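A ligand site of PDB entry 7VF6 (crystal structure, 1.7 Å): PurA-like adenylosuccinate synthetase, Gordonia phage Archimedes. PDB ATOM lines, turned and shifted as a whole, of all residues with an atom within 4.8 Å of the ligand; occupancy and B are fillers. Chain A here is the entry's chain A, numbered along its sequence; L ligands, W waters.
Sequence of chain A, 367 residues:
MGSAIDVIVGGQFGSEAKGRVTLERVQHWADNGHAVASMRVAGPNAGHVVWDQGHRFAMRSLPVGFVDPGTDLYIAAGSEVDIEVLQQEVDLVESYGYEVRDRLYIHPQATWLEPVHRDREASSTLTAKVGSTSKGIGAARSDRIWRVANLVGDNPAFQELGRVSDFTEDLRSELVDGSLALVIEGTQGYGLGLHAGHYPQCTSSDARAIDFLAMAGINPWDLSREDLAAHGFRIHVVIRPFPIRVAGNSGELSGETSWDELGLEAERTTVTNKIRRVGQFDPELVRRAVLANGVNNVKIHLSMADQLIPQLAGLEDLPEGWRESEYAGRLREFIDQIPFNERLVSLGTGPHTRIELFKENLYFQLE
OD1 of Asp 306 sits at hydrogen-bond distance from N3 of the ligand (2.6 Å).
O2 of the ligand is in hydrogen-bond range of N of Lys 18 (2.8 Å).
An oxygen (O2) of the ligand lies within salt-bridge range of the side-chain amino group (NZ) of Lys 18, 2.8 Å away.
The backbone NH (N) of Gly 19 sits at hydrogen-bond distance from an oxygen (O1) of the ligand.
O of Gly 47 lies close to O6 of the ligand.
A nitrogen (N2) of the ligand sits at hydrogen-bond distance from the guanidinium group (NE) of Arg 20 (2.9 Å).
An oxygen (O2) of the ligand lies within hydrogen-bond range of the backbone NH (N) of Ala 17, 3.0 Å away.
N of Met 304 sits at hydrogen-bond distance from O11 of the ligand, at 3.0 Å.
O5 of the ligand is in hydrogen-bond range of N of Val 49 (3.0 Å).
The backbone NH (N) of Gly 350 sits at hydrogen-bond distance from an oxygen (O11) of the ligand, at 3.3 Å.
An oxygen (O2) of the ligand lies within hydrogen-bond range of the backbone NH (N) of Glu 16 (3.3 Å).
The guanidinium group (NH2) of Arg 56 is in hydrogen-bond range of an oxygen (O9) of the ligand, at 3.3 Å.
O11 of the ligand is in hydrogen-bond range of N of Thr 349 (3.4 Å).
The guanidinium group (NH2) of Arg 276 lies within salt-bridge range of an oxygen (O6) of the ligand (3.6 Å).
NZ of Lys 18 is in salt-bridge range of OE1 of Glu 16, 3.0 Å away.
The guanidinium group (NH2) of Arg 20 sits at hydrogen-bond distance from the side-chain hydroxyl (OG) of Ser 303, 2.7 Å away.
The guanidinium group of Arg 240 lies close to the side-chain sulfur of Met 304 (3.6 Å).
The side-chain hydroxyl (OG1) of Thr 353 sits at hydrogen-bond distance from the backbone NH (N) of Gly 350, at 3.4 Å.
OG of Ser 15 sits at hydrogen-bond distance from NH2 of Arg 276 (3.1 Å).
The backbone carbonyl oxygen (O) of Ser 15 sits at hydrogen-bond distance from the guanidinium group (NH1) of Arg 240 (2.9 Å).
O of Glu 16 lies within hydrogen-bond range of OG of Ser 303 (2.8 Å).
OG1 of Thr 353 is in hydrogen-bond range of OG1 of Thr 349 (2.8 Å).
Ser 15 touches the ligand.
CD2 of His 48 touches O3 of the ligand, 3.3 Å away.
C of Gly 348 touches O11 of the ligand (3.2 Å).
Pro 351 touches the ligand.
Hydrophobic or aromatic side chains within 4 Å of the ligand: Ala 17, His 48, Val 49, Met 304 and Pro 351.
17 residues have an atom within 4 Å of the ligand: Ser 15, Glu 16, Ala 17, Lys 18, Gly 19, Arg 20, Gly 47, His 48, Val 49, Arg 56, Arg 276, Met 304, Asp 306, Gly 348, Thr 349, Gly 350 and Pro 351.
Along chain A the residues within 4 Å of the ligand span positions 15 to 351.
Water W2 lies within hydrogen-bond range of an oxygen (O3) of the ligand, the side-chain amino group (NZ) of Lys 18 and the backbone NH (N) of Ser 15.
Water W5 lies within hydrogen-bond range of O10 of the ligand (2.7 Å), NE of Arg 56 (2.9 Å) and NE1 of Trp 51 (2.9 Å).
Water W6 bridges an oxygen (O9) of the ligand (2.7 Å) and the guanidinium group of Arg 276 (3.0 Å).
Water W1 lies within hydrogen-bond range of the backbone carbonyl oxygen of Pro 351 (2.7 Å), the backbone carbonyl oxygen of Val 49 (2.8 Å) and an oxygen (O10) of the ligand (2.8 Å).
Water W4 lies within hydrogen-bond range of the backbone carbonyl oxygen of Val 49 (2.7 Å), an oxygen (O5) of the ligand (2.8 Å) and the backbone NH of Arg 20 (3.0 Å).
Water W3 lies within hydrogen-bond range of O8 of the ligand, NE2 of Gln 307 and SD of Met 304.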
ATOM      1  N   SER A  15      35.403 -15.380   1.824  1.00  0.00           N
ATOM      2  CA  SER A  15      34.112 -15.006   2.400  1.00  0.00           C
ATOM      3  C   SER A  15      32.944 -15.485   1.540  1.00  0.00           C
ATOM      4  O   SER A  15      31.905 -14.824   1.442  1.00  0.00           O
ATOM      5  CB  SER A  15      34.024 -13.505   2.652  1.00  0.00           C
ATOM      6  OG  SER A  15      35.110 -13.059   3.447  1.00  0.00           O
ATOM      7  N   GLU A  16      33.108 -16.652   0.941  1.00  0.00           N
ATOM      8  CA  GLU A  16      32.024 -17.216   0.140  1.00  0.00           C
ATOM      9  C   GLU A  16      31.016 -17.990   0.985  1.00  0.00           C
ATOM     10  O   GLU A  16      29.921 -18.274   0.500  1.00  0.00           O
ATOM     11  CB  GLU A  16      32.604 -18.116  -0.960  1.00  0.00           C
ATOM     12  CG  GLU A  16      33.616 -17.416  -1.887  1.00  0.00           C
ATOM     13  CD  GLU A  16      35.079 -17.642  -1.455  1.00  0.00           C
ATOM     14  OE1 GLU A  16      35.313 -18.009  -0.284  1.00  0.00           O
ATOM     15  OE2 GLU A  16      35.995 -17.438  -2.285  1.00  0.00           O
ATOM     16  N   ALA A  17      31.346 -18.266   2.254  1.00  0.00           N
ATOM     17  CA  ALA A  17      30.508 -18.946   3.257  1.00  0.00           C
ATOM     18  C   ALA A  17      30.977 -20.386   3.434  1.00  0.00           C
ATOM     19  O   ALA A  17      30.168 -21.318   3.536  1.00  0.00           O
ATOM     20  CB  ALA A  17      29.021 -18.893   2.914  1.00  0.00           C
ATOM     21  N   LYS A  18      32.292 -20.564   3.473  1.00  0.00           N
ATOM     22  CA  LYS A  18      32.858 -21.865   3.798  1.00  0.00           C
ATOM     23  C   LYS A  18      32.482 -22.292   5.213  1.00  0.00           C
ATOM     24  O   LYS A  18      32.320 -23.489   5.468  1.00  0.00           O
ATOM     25  CB  LYS A  18      34.376 -21.807   3.632  1.00  0.00           C
ATOM     26  CG  LYS A  18      34.771 -21.549   2.176  1.00  0.00           C
ATOM     27  CD  LYS A  18      36.285 -21.461   2.011  1.00  0.00           C
ATOM     28  CE  LYS A  18      36.887 -20.271   2.764  1.00  0.00           C
ATOM     29  NZ  LYS A  18      36.290 -18.934   2.353  1.00  0.00           N
ATOM     30  N   GLY A  19      32.337 -21.339   6.140  1.00  0.00           N
ATOM     31  CA  GLY A  19      31.892 -21.725   7.471  1.00  0.00           C
ATOM     32  C   GLY A  19      30.532 -22.417   7.431  1.00  0.00           C
ATOM     33  O   GLY A  19      30.365 -23.511   7.979  1.00  0.00           O
ATOM     34  N   ARG A  20      29.566 -21.806   6.754  1.00  0.00           N
ATOM     35  CA  ARG A  20      28.238 -22.412   6.660  1.00  0.00           C
ATOM     36  C   ARG A  20      28.313 -23.791   6.013  1.00  0.00           C
ATOM     37  O   ARG A  20      27.717 -24.756   6.519  1.00  0.00           O
ATOM     38  CB  ARG A  20      27.289 -21.523   5.859  1.00  0.00           C
ATOM     39  CG  ARG A  20      25.903 -22.141   5.700  1.00  0.00           C
ATOM     40  CD  ARG A  20      24.975 -21.269   4.863  1.00  0.00           C
ATOM     41  NE  ARG A  20      25.509 -20.983   3.537  1.00  0.00           N
ATOM     42  CZ  ARG A  20      25.479 -21.834   2.512  1.00  0.00           C
ATOM     43  NH1 ARG A  20      24.950 -23.048   2.670  1.00  0.00           N
ATOM     44  NH2 ARG A  20      25.993 -21.491   1.345  1.00  0.00           N
ATOM     45  N   GLY A  47      37.799 -15.201   9.421  1.00  0.00           N
ATOM     46  CA  GLY A  47      36.781 -15.792  10.282  1.00  0.00           C
ATOM     47  C   GLY A  47      35.787 -16.551   9.435  1.00  0.00           C
ATOM     48  O   GLY A  47      35.465 -16.146   8.310  1.00  0.00           O
ATOM     49  N   HIS A  48      35.289 -17.663   9.974  1.00  0.00           N
ATOM     50  CA  HIS A  48      34.279 -18.476   9.301  1.00  0.00           C
ATOM     51  C   HIS A  48      33.031 -18.451  10.162  1.00  0.00           C
ATOM     52  O   HIS A  48      33.060 -18.907  11.310  1.00  0.00           O
ATOM     53  CB  HIS A  48      34.758 -19.902   9.086  1.00  0.00           C
ATOM     54  CG  HIS A  48      36.001 -20.013   8.257  1.00  0.00           C
ATOM     55  ND1 HIS A  48      36.781 -21.151   8.241  1.00  0.00           N
ATOM     56  CD2 HIS A  48      36.593 -19.127   7.423  1.00  0.00           C
ATOM     57  CE1 HIS A  48      37.810 -20.956   7.425  1.00  0.00           C
ATOM     58  NE2 HIS A  48      37.729 -19.743   6.922  1.00  0.00           N
ATOM     59  N   VAL A  49      31.929 -17.931   9.619  1.00  0.00           N
ATOM     60  CA  VAL A  49      30.745 -17.637  10.423  1.00  0.00           C
ATOM     61  C   VAL A  49      29.753 -18.792  10.329  1.00  0.00           C
ATOM     62  O   VAL A  49      29.365 -19.206   9.222  1.00  0.00           O
ATOM     63  CB  VAL A  49      30.094 -16.324   9.983  1.00  0.00           C
ATOM     64  CG1 VAL A  49      28.864 -16.055  10.866  1.00  0.00           C
ATOM     65  CG2 VAL A  49      31.092 -15.181  10.076  1.00  0.00           C
ATOM     66  N   TRP A  51      26.053 -20.228  12.569  1.00  0.00           N
ATOM     67  CA  TRP A  51      25.020 -19.923  13.558  1.00  0.00           C
ATOM     68  C   TRP A  51      24.588 -21.219  14.234  1.00  0.00           C
ATOM     69  O   TRP A  51      24.499 -22.265  13.586  1.00  0.00           O
ATOM     70  CB  TRP A  51      23.800 -19.251  12.922  1.00  0.00           C
ATOM     71  CG  TRP A  51      23.978 -17.807  12.528  1.00  0.00           C
ATOM     72  CD1 TRP A  51      24.729 -17.316  11.485  1.00  0.00           C
ATOM     73  CD2 TRP A  51      23.353 -16.668  13.132  1.00  0.00           C
ATOM     74  NE1 TRP A  51      24.623 -15.943  11.435  1.00  0.00           N
ATOM     75  CE2 TRP A  51      23.788 -15.520  12.435  1.00  0.00           C
ATOM     76  CE3 TRP A  51      22.483 -16.510  14.216  1.00  0.00           C
ATOM     77  CZ2 TRP A  51      23.374 -14.236  12.780  1.00  0.00           C
ATOM     78  CZ3 TRP A  51      22.071 -15.233  14.554  1.00  0.00           C
ATOM     79  CH2 TRP A  51      22.514 -14.110  13.840  1.00  0.00           C
ATOM     80  N   ARG A  56      25.628 -16.273  16.796  1.00  0.00           N
ATOM     81  CA  ARG A  56      26.512 -16.145  15.632  1.00  0.00           C
ATOM     82  C   ARG A  56      27.949 -16.284  16.092  1.00  0.00           C
ATOM     83  O   ARG A  56      28.401 -15.523  16.957  1.00  0.00           O
ATOM     84  CB  ARG A  56      26.297 -14.793  14.952  1.00  0.00           C
ATOM     85  CG  ARG A  56      27.140 -14.534  13.724  1.00  0.00           C
ATOM     86  CD  ARG A  56      26.872 -13.120  13.220  1.00  0.00           C
ATOM     87  NE  ARG A  56      27.438 -12.843  11.907  1.00  0.00           N
ATOM     88  CZ  ARG A  56      28.664 -12.384  11.701  1.00  0.00           C
ATOM     89  NH1 ARG A  56      29.466 -12.155  12.738  1.00  0.00           N
ATOM     90  NH2 ARG A  56      29.085 -12.141  10.473  1.00  0.00           N
ATOM     91  N   ARG A 240      29.948 -17.058  -4.430  1.00  0.00           N
ATOM     92  CA  ARG A 240      28.846 -16.149  -4.168  1.00  0.00           C
ATOM     93  C   ARG A 240      28.576 -15.314  -5.422  1.00  0.00           C
ATOM     94  O   ARG A 240      29.454 -15.158  -6.270  1.00  0.00           O
ATOM     95  CB  ARG A 240      29.124 -15.231  -2.963  1.00  0.00           C
ATOM     96  CG  ARG A 240      30.500 -14.583  -2.948  1.00  0.00           C
ATOM     97  CD  ARG A 240      30.736 -13.885  -1.604  1.00  0.00           C
ATOM     98  NE  ARG A 240      29.843 -12.735  -1.432  1.00  0.00           N
ATOM     99  CZ  ARG A 240      29.634 -12.113  -0.279  1.00  0.00           C
ATOM    100  NH1 ARG A 240      30.232 -12.522   0.828  1.00  0.00           N
ATOM    101  NH2 ARG A 240      28.798 -11.076  -0.240  1.00  0.00           N
ATOM    102  N   THR A 270      35.508 -10.172   9.092  1.00  0.00           N
ATOM    103  CA  THR A 270      35.489 -10.627  10.482  1.00  0.00           C
ATOM    104  C   THR A 270      36.714 -10.172  11.252  1.00  0.00           C
ATOM    105  O   THR A 270      36.602  -9.715  12.402  1.00  0.00           O
ATOM    106  CB  THR A 270      35.392 -12.156  10.553  1.00  0.00           C
ATOM    107  OG1 THR A 270      34.022 -12.558  10.439  1.00  0.00           O
ATOM    108  CG2 THR A 270      35.941 -12.659  11.888  1.00  0.00           C
ATOM    109  N   ARG A 276      33.793  -4.578   3.336  1.00  0.00           N
ATOM    110  CA  ARG A 276      34.210  -5.335   2.170  1.00  0.00           C
ATOM    111  C   ARG A 276      33.948  -4.549   0.892  1.00  0.00           C
ATOM    112  O   ARG A 276      32.937  -3.847   0.763  1.00  0.00           O
ATOM    113  CB  ARG A 276      33.446  -6.667   2.102  1.00  0.00           C
ATOM    114  CG  ARG A 276      33.875  -7.705   3.130  1.00  0.00           C
ATOM    115  CD  ARG A 276      32.992  -8.961   3.072  1.00  0.00           C
ATOM    116  NE  ARG A 276      33.457  -9.991   3.995  1.00  0.00           N
ATOM    117  CZ  ARG A 276      32.666 -10.853   4.620  1.00  0.00           C
ATOM    118  NH1 ARG A 276      31.356 -10.836   4.426  1.00  0.00           N
ATOM    119  NH2 ARG A 276      33.195 -11.745   5.450  1.00  0.00           N
ATOM    120  N   SER A 303      26.502 -19.976  -2.643  1.00  0.00           N
ATOM    121  CA  SER A 303      26.074 -19.291  -1.444  1.00  0.00           C
ATOM    122  C   SER A 303      25.346 -18.010  -1.804  1.00  0.00           C
ATOM    123  O   SER A 303      25.525 -17.445  -2.879  1.00  0.00           O
ATOM    124  CB  SER A 303      27.259 -18.930  -0.537  1.00  0.00           C
ATOM    125  OG  SER A 303      27.871 -20.076  -0.006  1.00  0.00           O
ATOM    126  N   MET A 304      24.524 -17.533  -0.860  1.00  0.00           N
ATOM    127  CA  MET A 304      23.884 -16.223  -0.981  1.00  0.00           C
ATOM    128  C   MET A 304      23.074 -16.107  -2.269  1.00  0.00           C
ATOM    129  O   MET A 304      23.032 -15.071  -2.920  1.00  0.00           O
ATOM    130  CB  MET A 304      24.920 -15.096  -0.869  1.00  0.00           C
ATOM    131  CG  MET A 304      25.406 -14.890   0.572  1.00  0.00           C
ATOM    132  SD  MET A 304      26.990 -14.055   0.725  1.00  0.00           S
ATOM    133  CE  MET A 304      28.095 -15.439   1.032  1.00  0.00           C
ATOM    134  N   ASP A 306      20.116 -15.946  -2.012  1.00  0.00           N
ATOM    135  CA  ASP A 306      19.107 -14.994  -1.550  1.00  0.00           C
ATOM    136  C   ASP A 306      19.542 -13.548  -1.773  1.00  0.00           C
ATOM    137  O   ASP A 306      18.681 -12.656  -1.762  1.00  0.00           O
ATOM    138  CB  ASP A 306      18.797 -15.222  -0.067  1.00  0.00           C
ATOM    139  CG  ASP A 306      20.022 -15.100   0.824  1.00  0.00           C
ATOM    140  OD1 ASP A 306      20.979 -15.892   0.639  1.00  0.00           O
ATOM    141  OD2 ASP A 306      20.033 -14.224   1.708  1.00  0.00           O
ATOM    142  N   GLN A 307      20.838 -13.285  -1.974  1.00  0.00           N
ATOM    143  CA  GLN A 307      21.232 -11.941  -2.368  1.00  0.00           C
ATOM    144  C   GLN A 307      20.900 -11.680  -3.835  1.00  0.00           C
ATOM    145  O   GLN A 307      20.597 -10.546  -4.202  1.00  0.00           O
ATOM    146  CB  GLN A 307      22.721 -11.719  -2.124  1.00  0.00           C
ATOM    147  CG  GLN A 307      23.060 -11.643  -0.663  1.00  0.00           C
ATOM    148  CD  GLN A 307      24.484 -11.224  -0.410  1.00  0.00           C
ATOM    149  OE1 GLN A 307      25.337 -11.288  -1.300  1.00  0.00           O
ATOM    150  NE2 GLN A 307      24.751 -10.765   0.810  1.00  0.00           N
ATOM    151  N   GLY A 348      22.672 -21.605  -1.260  1.00  0.00           N
ATOM    152  CA  GLY A 348      22.580 -20.985   0.059  1.00  0.00           C
ATOM    153  C   GLY A 348      21.498 -19.915   0.071  1.00  0.00           C
ATOM    154  O   GLY A 348      21.389 -19.099  -0.854  1.00  0.00           O
ATOM    155  N   THR A 349      20.667 -19.916   1.124  1.00  0.00           N
ATOM    156  CA  THR A 349      19.566 -18.956   1.238  1.00  0.00           C
ATOM    157  C   THR A 349      19.621 -18.114   2.499  1.00  0.00           C
ATOM    158  O   THR A 349      18.707 -17.325   2.746  1.00  0.00           O
ATOM    159  CB  THR A 349      18.211 -19.684   1.189  1.00  0.00           C
ATOM    160  OG1 THR A 349      18.119 -20.568   2.309  1.00  0.00           O
ATOM    161  CG2 THR A 349      18.067 -20.486  -0.107  1.00  0.00           C
ATOM    162  N   GLY A 350      20.646 -18.271   3.316  1.00  0.00           N
ATOM    163  CA  GLY A 350      20.819 -17.473   4.501  1.00  0.00           C
ATOM    164  C   GLY A 350      22.002 -18.012   5.256  1.00  0.00           C
ATOM    165  O   GLY A 350      22.631 -19.007   4.848  1.00  0.00           O
ATOM    166  N   PRO A 351      22.344 -17.375   6.366  1.00  0.00           N
ATOM    167  CA  PRO A 351      23.538 -17.781   7.116  1.00  0.00           C
ATOM    168  C   PRO A 351      23.471 -19.205   7.655  1.00  0.00           C
ATOM    169  O   PRO A 351      24.513 -19.748   8.023  1.00  0.00           O
ATOM    170  CB  PRO A 351      23.612 -16.756   8.253  1.00  0.00           C
ATOM    171  CG  PRO A 351      22.792 -15.549   7.757  1.00  0.00           C
ATOM    172  CD  PRO A 351      21.714 -16.134   6.896  1.00  0.00           C
ATOM    173  N   THR A 353      20.786 -21.645   6.231  1.00  0.00           N
ATOM    174  CA  THR A 353      19.784 -22.371   5.460  1.00  0.00           C
ATOM    175  C   THR A 353      20.277 -22.551   4.032  1.00  0.00           C
ATOM    176  O   THR A 353      21.041 -21.732   3.518  1.00  0.00           O
ATOM    177  CB  THR A 353      18.421 -21.642   5.450  1.00  0.00           C
ATOM    178  OG1 THR A 353      18.577 -20.290   5.012  1.00  0.00           O
ATOM    179  CG2 THR A 353      17.781 -21.677   6.825  1.00  0.00           C
HETATM  180  P1  LIG L   1      33.872 -17.765   4.989  1.00  0.00           P
HETATM  181  O1  LIG L   1      33.507 -18.825   5.886  1.00  0.00           O
HETATM  182  O2  LIG L   1      33.969 -18.302   3.719  1.00  0.00           O
HETATM  183  O3  LIG L   1      35.076 -17.081   5.367  1.00  0.00           O
HETATM  184  O4  LIG L   1      32.712 -16.657   4.838  1.00  0.00           O
HETATM  185  P2  LIG L   1      32.276 -15.725   6.052  1.00  0.00           P
HETATM  186  O5  LIG L   1      31.494 -16.523   6.953  1.00  0.00           O
HETATM  187  O6  LIG L   1      33.347 -15.088   6.658  1.00  0.00           O
HETATM  188  O7  LIG L   1      31.305 -14.643   5.453  1.00  0.00           O
HETATM  189  C1  LIG L   1      30.161 -14.982   4.652  1.00  0.00           C
HETATM  190  C2  LIG L   1      28.796 -14.466   5.188  1.00  0.00           C
HETATM  191  O8  LIG L   1      27.682 -14.434   4.764  1.00  0.00           O
HETATM  192  C3  LIG L   1      28.681 -14.550   6.843  1.00  0.00           C
HETATM  193  O9  LIG L   1      28.206 -13.366   7.485  1.00  0.00           O
HETATM  194  C4  LIG L   1      27.782 -15.542   6.890  1.00  0.00           C
HETATM  195  O10 LIG L   1      27.012 -15.685   8.177  1.00  0.00           O
HETATM  196  C5  LIG L   1      26.879 -15.341   5.635  1.00  0.00           C
HETATM  197  N1  LIG L   1      26.177 -16.263   4.943  1.00  0.00           N
HETATM  198  C6  LIG L   1      26.592 -17.495   4.700  1.00  0.00           C
HETATM  199  N2  LIG L   1      25.800 -18.086   3.810  1.00  0.00           N
HETATM  200  C7  LIG L   1      24.914 -17.267   3.433  1.00  0.00           C
HETATM  201  C8  LIG L   1      23.743 -17.384   2.453  1.00  0.00           C
HETATM  202  O11 LIG L   1      23.599 -18.353   1.915  1.00  0.00           O
HETATM  203  N3  LIG L   1      22.923 -16.194   2.340  1.00  0.00           N
HETATM  204  C9  LIG L   1      23.244 -15.049   3.047  1.00  0.00           C
HETATM  205  N4  LIG L   1      22.502 -13.831   3.014  1.00  0.00           N
HETATM  206  N5  LIG L   1      24.368 -15.024   3.937  1.00  0.00           N
HETATM  207  C10 LIG L   1      25.160 -16.184   4.088  1.00  0.00           C
HETATM  208  O   HOH W   1      26.832 -18.418   8.481  1.00  0.00           O
HETATM  209  O   HOH W   2      37.332 -17.055   4.173  1.00  0.00           O
HETATM  210  O   HOH W   3      26.310 -11.984   3.640  1.00  0.00           O
HETATM  211  O   HOH W   4      29.902 -18.813   6.625  1.00  0.00           O
HETATM  212  O   HOH W   5      25.803 -13.871   9.700  1.00  0.00           O
HETATM  213  O   HOH W   6      29.671 -11.166   6.910  1.00  0.00           O
